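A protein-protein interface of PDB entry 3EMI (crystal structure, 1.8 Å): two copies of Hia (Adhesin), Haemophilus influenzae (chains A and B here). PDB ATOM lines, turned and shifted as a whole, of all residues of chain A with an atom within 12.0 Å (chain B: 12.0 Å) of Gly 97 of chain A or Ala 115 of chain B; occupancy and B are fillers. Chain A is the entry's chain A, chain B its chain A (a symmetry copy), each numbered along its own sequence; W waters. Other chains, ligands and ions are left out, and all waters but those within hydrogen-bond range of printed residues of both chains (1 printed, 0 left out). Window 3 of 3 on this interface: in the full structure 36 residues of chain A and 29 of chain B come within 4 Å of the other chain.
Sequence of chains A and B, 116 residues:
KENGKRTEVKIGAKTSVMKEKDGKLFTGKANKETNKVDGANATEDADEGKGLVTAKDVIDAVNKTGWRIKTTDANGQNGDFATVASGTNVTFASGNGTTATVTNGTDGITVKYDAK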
ATOM      1  N   PHE A  92      22.841  -7.109  31.994  1.00  0.00           N
ATOM      2  CA  PHE A  92      23.247  -6.171  30.957  1.00  0.00           C
ATOM      3  C   PHE A  92      24.628  -6.578  30.455  1.00  0.00           C
ATOM      4  O   PHE A  92      25.637  -6.313  31.097  1.00  0.00           O
ATOM      5  CB  PHE A  92      23.185  -4.734  31.475  1.00  0.00           C
ATOM      6  CG  PHE A  92      21.786  -4.268  31.722  1.00  0.00           C
ATOM      7  CD1 PHE A  92      21.075  -3.617  30.726  1.00  0.00           C
ATOM      8  CD2 PHE A  92      21.151  -4.547  32.924  1.00  0.00           C
ATOM      9  CE1 PHE A  92      19.767  -3.224  30.937  1.00  0.00           C
ATOM     10  CE2 PHE A  92      19.839  -4.152  33.138  1.00  0.00           C
ATOM     11  CZ  PHE A  92      19.149  -3.491  32.143  1.00  0.00           C
ATOM     12  N   ALA A  93      24.652  -7.264  29.315  1.00  0.00           N
ATOM     13  CA  ALA A  93      25.865  -7.901  28.823  1.00  0.00           C
ATOM     14  C   ALA A  93      26.685  -6.928  28.007  1.00  0.00           C
ATOM     15  O   ALA A  93      26.136  -6.102  27.287  1.00  0.00           O
ATOM     16  CB  ALA A  93      25.514  -9.131  27.976  1.00  0.00           C
ATOM     17  N   SER A  94      28.003  -7.037  28.107  1.00  0.00           N
ATOM     18  CA  SER A  94      28.886  -6.289  27.227  1.00  0.00           C
ATOM     19  C   SER A  94      28.697  -6.827  25.816  1.00  0.00           C
ATOM     20  O   SER A  94      28.344  -7.995  25.634  1.00  0.00           O
ATOM     21  CB  SER A  94      30.340  -6.457  27.665  1.00  0.00           C
ATOM     22  OG  SER A  94      30.524  -6.006  29.002  1.00  0.00           O
ATOM     23  N   GLY A  95      28.926  -5.981  24.816  1.00  0.00           N
ATOM     24  CA  GLY A  95      28.733  -6.393  23.442  1.00  0.00           C
ATOM     25  C   GLY A  95      29.928  -6.103  22.557  1.00  0.00           C
ATOM     26  O   GLY A  95      31.018  -5.775  23.039  1.00  0.00           O
ATOM     27  N   ASN A  96      29.720  -6.229  21.253  1.00  0.00           N
ATOM     28  CA  ASN A  96      30.771  -5.930  20.298  1.00  0.00           C
ATOM     29  C   ASN A  96      31.256  -4.496  20.457  1.00  0.00           C
ATOM     30  O   ASN A  96      30.532  -3.552  20.162  1.00  0.00           O
ATOM     31  CB  ASN A  96      30.279  -6.186  18.872  1.00  0.00           C
ATOM     32  CG  ASN A  96      30.103  -7.664  18.579  1.00  0.00           C
ATOM     33  OD1 ASN A  96      30.739  -8.513  19.213  1.00  0.00           O
ATOM     34  ND2 ASN A  96      29.236  -7.983  17.622  1.00  0.00           N
ATOM     35  N   GLY A  97      32.476  -4.338  20.955  1.00  0.00           N
ATOM     36  CA  GLY A  97      33.065  -3.017  21.092  1.00  0.00           C
ATOM     37  C   GLY A  97      32.431  -2.177  22.184  1.00  0.00           C
ATOM     38  O   GLY A  97      32.522  -0.948  22.164  1.00  0.00           O
ATOM     39  N   THR A  98      31.780  -2.829  23.143  1.00  0.00           N
ATOM     40  CA  THR A  98      31.242  -2.111  24.295  1.00  0.00           C
ATOM     41  C   THR A  98      31.532  -2.869  25.583  1.00  0.00           C
ATOM     42  O   THR A  98      31.794  -4.073  25.571  1.00  0.00           O
ATOM     43  CB  THR A  98      29.717  -1.911  24.211  1.00  0.00           C
ATOM     44  OG1 THR A  98      29.066  -3.178  24.369  1.00  0.00           O
ATOM     45  CG2 THR A  98      29.320  -1.268  22.871  1.00  0.00           C
ATOM     46  N   THR A  99      31.474  -2.157  26.698  1.00  0.00           N
ATOM     47  CA  THR A  99      31.681  -2.772  27.993  1.00  0.00           C
ATOM     48  C   THR A  99      30.577  -2.335  28.938  1.00  0.00           C
ATOM     49  O   THR A  99      30.356  -1.138  29.126  1.00  0.00           O
ATOM     50  CB  THR A  99      33.034  -2.372  28.578  1.00  0.00           C
ATOM     51  OG1 THR A  99      34.075  -2.776  27.675  1.00  0.00           O
ATOM     52  CG2 THR A  99      33.250  -3.035  29.930  1.00  0.00           C
ATOM     53  N   ALA A 100      29.881  -3.308  29.518  1.00  0.00           N
ATOM     54  CA  ALA A 100      28.819  -3.018  30.476  1.00  0.00           C
ATOM     55  C   ALA A 100      29.328  -3.142  31.903  1.00  0.00           C
ATOM     56  O   ALA A 100      30.062  -4.075  32.239  1.00  0.00           O
ATOM     57  CB  ALA A 100      27.635  -3.952  30.260  1.00  0.00           C
ATOM     58  N   THR A 101      28.924  -2.193  32.737  1.00  0.00           N
ATOM     59  CA  THR A 101      29.154  -2.286  34.164  1.00  0.00           C
ATOM     60  C   THR A 101      27.846  -1.983  34.869  1.00  0.00           C
ATOM     61  O   THR A 101      27.050  -1.156  34.405  1.00  0.00           O
ATOM     62  CB  THR A 101      30.248  -1.312  34.634  1.00  0.00           C
ATOM     63  OG1 THR A 101      29.896   0.026  34.264  1.00  0.00           O
ATOM     64  CG2 THR A 101      31.561  -1.670  33.988  1.00  0.00           C
ATOM     65  N   LYS A 112      25.849   1.126  32.952  1.00  0.00           N
ATOM     66  CA  LYS A 112      26.627   1.945  32.037  1.00  0.00           C
ATOM     67  C   LYS A 112      27.225   1.096  30.930  1.00  0.00           C
ATOM     68  O   LYS A 112      27.662  -0.029  31.170  1.00  0.00           O
ATOM     69  CB  LYS A 112      27.732   2.684  32.790  1.00  0.00           C
ATOM     70  CG  LYS A 112      28.534   3.650  31.913  1.00  0.00           C
ATOM     71  CD  LYS A 112      29.330   4.624  32.750  1.00  0.00           C
ATOM     72  CE  LYS A 112      30.470   3.932  33.461  1.00  0.00           C
ATOM     73  NZ  LYS A 112      31.159   4.870  34.380  1.00  0.00           N
ATOM     74  N   TYR A 113      27.208   1.639  29.715  1.00  0.00           N
ATOM     75  CA  TYR A 113      27.916   1.054  28.585  1.00  0.00           C
ATOM     76  C   TYR A 113      29.009   2.022  28.143  1.00  0.00           C
ATOM     77  O   TYR A 113      28.745   3.203  27.925  1.00  0.00           O
ATOM     78  CB  TYR A 113      26.952   0.751  27.422  1.00  0.00           C
ATOM     79  CG  TYR A 113      26.231  -0.570  27.571  1.00  0.00           C
ATOM     80  CD1 TYR A 113      26.762  -1.733  27.022  1.00  0.00           C
ATOM     81  CD2 TYR A 113      25.034  -0.662  28.277  1.00  0.00           C
ATOM     82  CE1 TYR A 113      26.116  -2.951  27.163  1.00  0.00           C
ATOM     83  CE2 TYR A 113      24.385  -1.872  28.426  1.00  0.00           C
ATOM     84  CZ  TYR A 113      24.931  -3.013  27.871  1.00  0.00           C
ATOM     85  OH  TYR A 113      24.288  -4.220  28.006  1.00  0.00           O
ATOM     86  N   ASP A 114      30.238   1.523  28.060  1.00  0.00           N
ATOM     87  CA  ASP A 114      31.346   2.283  27.510  1.00  0.00           C
ATOM     88  C   ASP A 114      31.631   1.737  26.127  1.00  0.00           C
ATOM     89  O   ASP A 114      31.423   0.556  25.874  1.00  0.00           O
ATOM     90  CB  ASP A 114      32.605   2.092  28.357  1.00  0.00           C
ATOM     91  CG  ASP A 114      32.474   2.676  29.743  1.00  0.00           C
ATOM     92  OD1 ASP A 114      31.988   3.819  29.867  1.00  0.00           O
ATOM     93  OD2 ASP A 114      32.874   1.991  30.708  1.00  0.00           O
ATOM     94  N   ALA A 115      32.114   2.590  25.231  1.00  0.00           N
ATOM     95  CA  ALA A 115      32.587   2.113  23.944  1.00  0.00           C
ATOM     96  C   ALA A 115      34.061   1.781  24.097  1.00  0.00           C
ATOM     97  O   ALA A 115      34.801   2.537  24.722  1.00  0.00           O
ATOM     98  CB  ALA A 115      32.382   3.181  22.865  1.00  0.00           C
ATOM     99  N   LYS A 116      34.485   0.645  23.553  1.00  0.00           N
ATOM    100  CA  LYS A 116      35.900   0.297  23.557  1.00  0.00           C
ATOM    101  C   LYS A 116      36.638   1.188  22.564  1.00  0.00           C
ATOM    102  O   LYS A 116      36.223   1.334  21.411  1.00  0.00           O
ATOM    103  CB  LYS A 116      36.097  -1.171  23.178  1.00  0.00           C
ATOM    104  CG  LYS A 116      35.563  -2.169  24.187  1.00  0.00           C
ATOM    105  CD  LYS A 116      35.696  -3.588  23.655  1.00  0.00           C
ATOM    106  CE  LYS A 116      35.271  -4.612  24.689  1.00  0.00           C
ATOM    107  NZ  LYS A 116      36.065  -4.459  25.939  1.00  0.00           N
ATOM    108  OXT LYS A 116      37.668   1.782  22.883  1.00  0.00           O
ATOM    109  N   ALA B  93      16.232   0.585  23.038  1.00  0.00           N
ATOM    110  CA  ALA B  93      16.271   0.900  21.617  1.00  0.00           C
ATOM    111  C   ALA B  93      17.698   0.952  21.122  1.00  0.00           C
ATOM    112  O   ALA B  93      18.589   1.398  21.834  1.00  0.00           O
ATOM    113  CB  ALA B  93      15.574   2.240  21.350  1.00  0.00           C
ATOM    114  N   SER B  94      17.911   0.509  19.889  1.00  0.00           N
ATOM    115  CA  SER B  94      19.200   0.689  19.240  1.00  0.00           C
ATOM    116  C   SER B  94      19.397   2.180  19.008  1.00  0.00           C
ATOM    117  O   SER B  94      18.423   2.923  18.861  1.00  0.00           O
ATOM    118  CB  SER B  94      19.235  -0.062  17.911  1.00  0.00           C
ATOM    119  OG  SER B  94      19.003  -1.452  18.105  1.00  0.00           O
ATOM    120  N   GLY B  95      20.650   2.622  18.978  1.00  0.00           N
ATOM    121  CA  GLY B  95      20.932   4.032  18.802  1.00  0.00           C
ATOM    122  C   GLY B  95      21.927   4.307  17.694  1.00  0.00           C
ATOM    123  O   GLY B  95      22.255   3.427  16.891  1.00  0.00           O
ATOM    124  N   ASN B  96      22.407   5.543  17.649  1.00  0.00           N
ATOM    125  CA  ASN B  96      23.405   5.921  16.666  1.00  0.00           C
ATOM    126  C   ASN B  96      24.646   5.047  16.791  1.00  0.00           C
ATOM    127  O   ASN B  96      25.379   5.135  17.769  1.00  0.00           O
ATOM    128  CB  ASN B  96      23.762   7.401  16.816  1.00  0.00           C
ATOM    129  CG  ASN B  96      22.633   8.314  16.373  1.00  0.00           C
ATOM    130  OD1 ASN B  96      21.789   7.924  15.559  1.00  0.00           O
ATOM    131  ND2 ASN B  96      22.607   9.532  16.908  1.00  0.00           N
ATOM    132  N   GLY B  97      24.860   4.183  15.807  1.00  0.00           N
ATOM    133  CA  GLY B  97      26.045   3.343  15.790  1.00  0.00           C
ATOM    134  C   GLY B  97      26.036   2.253  16.844  1.00  0.00           C
ATOM    135  O   GLY B  97      27.088   1.738  17.226  1.00  0.00           O
ATOM    136  N   THR B  98      24.849   1.897  17.329  1.00  0.00           N
ATOM    137  CA  THR B  98      24.734   0.775  18.258  1.00  0.00           C
ATOM    138  C   THR B  98      23.551  -0.109  17.887  1.00  0.00           C
ATOM    139  O   THR B  98      22.629   0.316  17.189  1.00  0.00           O
ATOM    140  CB  THR B  98      24.533   1.230  19.715  1.00  0.00           C
ATOM    141  OG1 THR B  98      23.230   1.812  19.851  1.00  0.00           O
ATOM    142  CG2 THR B  98      25.617   2.238  20.131  1.00  0.00           C
ATOM    143  N   THR B  99      23.578  -1.342  18.371  1.00  0.00           N
ATOM    144  CA  THR B  99      22.488  -2.265  18.132  1.00  0.00           C
ATOM    145  C   THR B  99      22.090  -2.921  19.442  1.00  0.00           C
ATOM    146  O   THR B  99      22.931  -3.507  20.125  1.00  0.00           O
ATOM    147  CB  THR B  99      22.895  -3.344  17.130  1.00  0.00           C
ATOM    148  OG1 THR B  99      23.283  -2.720  15.897  1.00  0.00           O
ATOM    149  CG2 THR B  99      21.740  -4.300  16.874  1.00  0.00           C
ATOM    150  N   ALA B 100      20.813  -2.807  19.791  1.00  0.00           N
ATOM    151  CA  ALA B 100      20.298  -3.426  21.008  1.00  0.00           C
ATOM    152  C   ALA B 100      19.630  -4.757  20.700  1.00  0.00           C
ATOM    153  O   ALA B 100      18.889  -4.886  19.722  1.00  0.00           O
ATOM    154  CB  ALA B 100      19.313  -2.496  21.705  1.00  0.00           C
ATOM    155  N   THR B 101      19.900  -5.740  21.549  1.00  0.00           N
ATOM    156  CA  THR B 101      19.183  -6.998  21.506  1.00  0.00           C
ATOM    157  C   THR B 101      18.737  -7.329  22.918  1.00  0.00           C
ATOM    158  O   THR B 101      19.437  -7.027  23.893  1.00  0.00           O
ATOM    159  CB  THR B 101      20.053  -8.135  20.944  1.00  0.00           C
ATOM    160  OG1 THR B 101      21.250  -8.260  21.721  1.00  0.00           O
ATOM    161  CG2 THR B 101      20.425  -7.833  19.516  1.00  0.00           C
ATOM    162  N   VAL B 111      20.068  -8.097  28.202  1.00  0.00           N
ATOM    163  CA  VAL B 111      20.097  -6.920  27.354  1.00  0.00           C
ATOM    164  C   VAL B 111      21.540  -6.739  26.903  1.00  0.00           C
ATOM    165  O   VAL B 111      22.479  -6.958  27.671  1.00  0.00           O
ATOM    166  CB  VAL B 111      19.655  -5.663  28.127  1.00  0.00           C
ATOM    167  CG1 VAL B 111      19.821  -4.413  27.267  1.00  0.00           C
ATOM    168  CG2 VAL B 111      18.217  -5.802  28.607  1.00  0.00           C
ATOM    169  N   LYS B 112      21.721  -6.350  25.650  1.00  0.00           N
ATOM    170  CA  LYS B 112      23.058  -6.137  25.121  1.00  0.00           C
ATOM    171  C   LYS B 112      23.058  -5.019  24.094  1.00  0.00           C
ATOM    172  O   LYS B 112      22.125  -4.897  23.301  1.00  0.00           O
ATOM    173  CB  LYS B 112      23.596  -7.425  24.499  1.00  0.00           C
ATOM    174  CG  LYS B 112      25.043  -7.312  24.008  1.00  0.00           C
ATOM    175  CD  LYS B 112      25.652  -8.673  23.770  1.00  0.00           C
ATOM    176  CE  LYS B 112      25.035  -9.347  22.566  1.00  0.00           C
ATOM    177  NZ  LYS B 112      25.547 -10.732  22.424  1.00  0.00           N
ATOM    178  N   TYR B 113      24.100  -4.193  24.142  1.00  0.00           N
ATOM    179  CA  TYR B 113      24.360  -3.198  23.112  1.00  0.00           C
ATOM    180  C   TYR B 113      25.673  -3.548  22.418  1.00  0.00           C
ATOM    181  O   TYR B 113      26.687  -3.765  23.076  1.00  0.00           O
ATOM    182  CB  TYR B 113      24.421  -1.779  23.711  1.00  0.00           C
ATOM    183  CG  TYR B 113      23.061  -1.145  23.890  1.00  0.00           C
ATOM    184  CD1 TYR B 113      22.508  -0.358  22.885  1.00  0.00           C
ATOM    185  CD2 TYR B 113      22.316  -1.350  25.049  1.00  0.00           C
ATOM    186  CE1 TYR B 113      21.256   0.217  23.032  1.00  0.00           C
ATOM    187  CE2 TYR B 113      21.066  -0.784  25.204  1.00  0.00           C
ATOM    188  CZ  TYR B 113      20.540  -0.005  24.193  1.00  0.00           C
ATOM    189  OH  TYR B 113      19.301   0.572  24.341  1.00  0.00           O
ATOM    190  N   ASP B 114      25.628  -3.646  21.092  1.00  0.00           N
ATOM    191  CA  ASP B 114      26.825  -3.824  20.291  1.00  0.00           C
ATOM    192  C   ASP B 114      27.128  -2.498  19.625  1.00  0.00           C
ATOM    193  O   ASP B 114      26.219  -1.733  19.331  1.00  0.00           O
ATOM    194  CB  ASP B 114      26.589  -4.856  19.188  1.00  0.00           C
ATOM    195  CG  ASP B 114      26.357  -6.248  19.727  1.00  0.00           C
ATOM    196  OD1 ASP B 114      27.113  -6.675  20.624  1.00  0.00           O
ATOM    197  OD2 ASP B 114      25.423  -6.918  19.239  1.00  0.00           O
ATOM    198  N   ALA B 115      28.405  -2.226  19.380  1.00  0.00           N
ATOM    199  CA  ALA B 115      28.769  -1.068  18.583  1.00  0.00           C
ATOM    200  C   ALA B 115      28.813  -1.512  17.132  1.00  0.00           C
ATOM    201  O   ALA B 115      29.331  -2.586  16.832  1.00  0.00           O
ATOM    202  CB  ALA B 115      30.128  -0.516  19.023  1.00  0.00           C
ATOM    203  N   LYS B 116      28.252  -0.708  16.235  1.00  0.00           N
ATOM    204  CA  LYS B 116      28.341  -1.000  14.810  1.00  0.00           C
ATOM    205  C   LYS B 116      29.765  -0.737  14.332  1.00  0.00           C
ATOM    206  O   LYS B 116      30.341   0.320  14.603  1.00  0.00           O
ATOM    207  CB  LYS B 116      27.364  -0.132  14.018  1.00  0.00           C
ATOM    208  CG  LYS B 116      25.898  -0.426  14.271  1.00  0.00           C
ATOM    209  CD  LYS B 116      25.019   0.574  13.535  1.00  0.00           C
ATOM    210  CE  LYS B 116      23.548   0.235  13.680  1.00  0.00           C
ATOM    211  NZ  LYS B 116      23.273  -1.144  13.191  1.00  0.00           N
ATOM    212  OXT LYS B 116      30.377  -1.570  13.662  1.00  0.00           O
HETATM  213  O   HOH W   1      28.050  -9.535  21.074  1.00  0.00           O
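Val 111 of chain B touches Phe 92 of chain A (O to CA, 3.5 Å).
Lys 112 of chain B touches Ala 93 of chain A (CG to O, 3.7 Å).
Lys 112 of chain B touches Ser 94 of chain A (CD to O, 3.3 Å).
Lys 112 of chain B touches Gly 95 of chain A.
CA of Gly 95 of chain A touches O of Tyr 113 of chain B, 3.4 Å away.
CA of Gly 95 of chain A touches OD1 of Asp 114 of chain B (3.3 Å).
Gly 97 of chain A touches Ala 115 of chain B (O to CB, 3.97 Å).
Thr 98 of chain A touches Ala 115 of chain B.
Lys 112 of chain B touches Tyr 113 of chain A (CA to OH, 3.7 Å).
Tyr 113 of chain B touches Tyr 113 of chain A (N to CE1, 3.8 Å).
Ala 93 of chain A touches Lys 112 of chain B, but with the chains exchanged Lys 112 of chain A does not touch Ala 93 of chain B (12.5 Å).
Asn 96 of chain A touches Asp 114 of chain B, but with the chains exchanged Asp 114 of chain A does not touch Asn 96 of chain B (11.0 Å).
Thr 98 of chain A touches Tyr 113 of chain B, but with the chains exchanged Tyr 113 of chain A does not touch Thr 98 of chain B (7.6 Å).
Thr 98 of chain A touches Ala 115 of chain B, but with the chains exchanged Ala 115 of chain A does not touch Thr 98 of chain B (7.4 Å).
14 positions are printed for both chains.
Of the 15 pairs that touch across the chains among the printed residues, 1 has its exchanged pair printed and touching as well.
Water W1 lies within hydrogen-bond range of the side-chain carboxylate (OD1) of Asp 114 of chain B, the side-chain amino group (NZ) of Lys 112 of chain B and the side-chain amide oxygen (OD1) of Asn 96 of chain A.
The backbone carbonyl oxygen (O) of Val 111 of chain B lies within hydrogen-bond range of the backbone NH (N) of Ala 93 of chain A (2.7 Å).
The side-chain carboxylate of Asp 114 of chain B is in hydrogen-bond range of the backbone NH of Asn 96 of chain A (2.7 Å).
The backbone carbonyl oxygen (O) of Asn 96 of chain A is in hydrogen-bond range of the backbone NH (N) of Ala 115 of chain B (2.6 Å).
The backbone carbonyl oxygen of Tyr 113 of chain B sits at hydrogen-bond distance from the side-chain hydroxyl of Thr 98 of chain A (2.8 Å).
OH of Tyr 113 of chain A is in hydrogen-bond range of O of Val 111 of chain B (3.3 Å).
Hydrophobic or aromatic side chains of chain A that line the printed part of chain B: Phe 92, Ala 93 and Tyr 113.
Along chain A the printed residues that touch a printed residue of chain B span positions 92 to 113.
Of the 15 printed residues of chain B, 5 touch a printed residue of chain A.
Printed residues of chain B that touch a printed residue of chain A: Val 111, Lys 112, Tyr 113, Asp 114 and Ala 115.
Hydrophobic or aromatic side chains of chain B within 4 Å of the printed part of chain A: Val 111, Tyr 113 and Ala 115.
Among the printed residues, no Asp or Glu carboxylate lies within 4 Å of a Lys or Arg side-chain nitrogen of the other chain.
O of Ala 93 of chain A lies within hydrogen-bond range of OH of Tyr 113 of chain A, at 2.7 Å.
OG of Ser 94 of chain A lies within hydrogen-bond range of N of Ala 100 of chain A.
The side-chain hydroxyl (OG1) of Thr 98 of chain A sits at hydrogen-bond distance from the backbone NH (N) of Gly 95 of chain A, 2.8 Å away.
The backbone carbonyl oxygen of Gly 97 of chain A lies within hydrogen-bond range of the backbone NH of Lys 116 of chain A (2.9 Å).
O of Ala 93 of chain B sits at hydrogen-bond distance from OH of Tyr 113 of chain B (2.7 Å).
The backbone NH (N) of Thr 99 of chain B lies within hydrogen-bond range of the backbone carbonyl oxygen (O) of Asp 114 of chain B, 2.8 Å away.
Of chain B, only Ala 115 comes within 4 Å of Gly 97 of chain A.
Ala 115 of chain B touches three residues of chain A.
Thr 98 of chain A touches two residues of chain B.
No residue of chain B comes within 4 Å of Thr 99 of chain A.
No residue of chain B comes within 4 Å of Ala 115 of chain A.
No residue of chain B comes within 4 Å of Lys 116 of chain A.
No residue of chain A comes within 4 Å of Gly 97 of chain B.
No residue of chain A comes within 4 Å of Thr 98 of chain B.
Thr 99 of chain B touches none of the printed residues of chain A.
Asp 114 of chain B touches just these residues of chain A: Gly 95 (3.3 Å) and Asn 96 (2.7 Å).
No residue of chain A comes within 4 Å of Lys 116 of chain B.
Of the printed residues of chain B, Ser 94 of chain A touches Lys 112 (3.3 Å).
Printed residues of chain A within 4 Å of Val 111 of chain B: Phe 92, Ala 93 and Tyr 113.
Of the printed residues of chain B, Tyr 113 of chain A touches Val 111, Lys 112 and Tyr 113.
Thr 101 of chain A touches none of the printed residues of chain B.
Gly 95 of chain B touches none of the printed residues of chain A.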
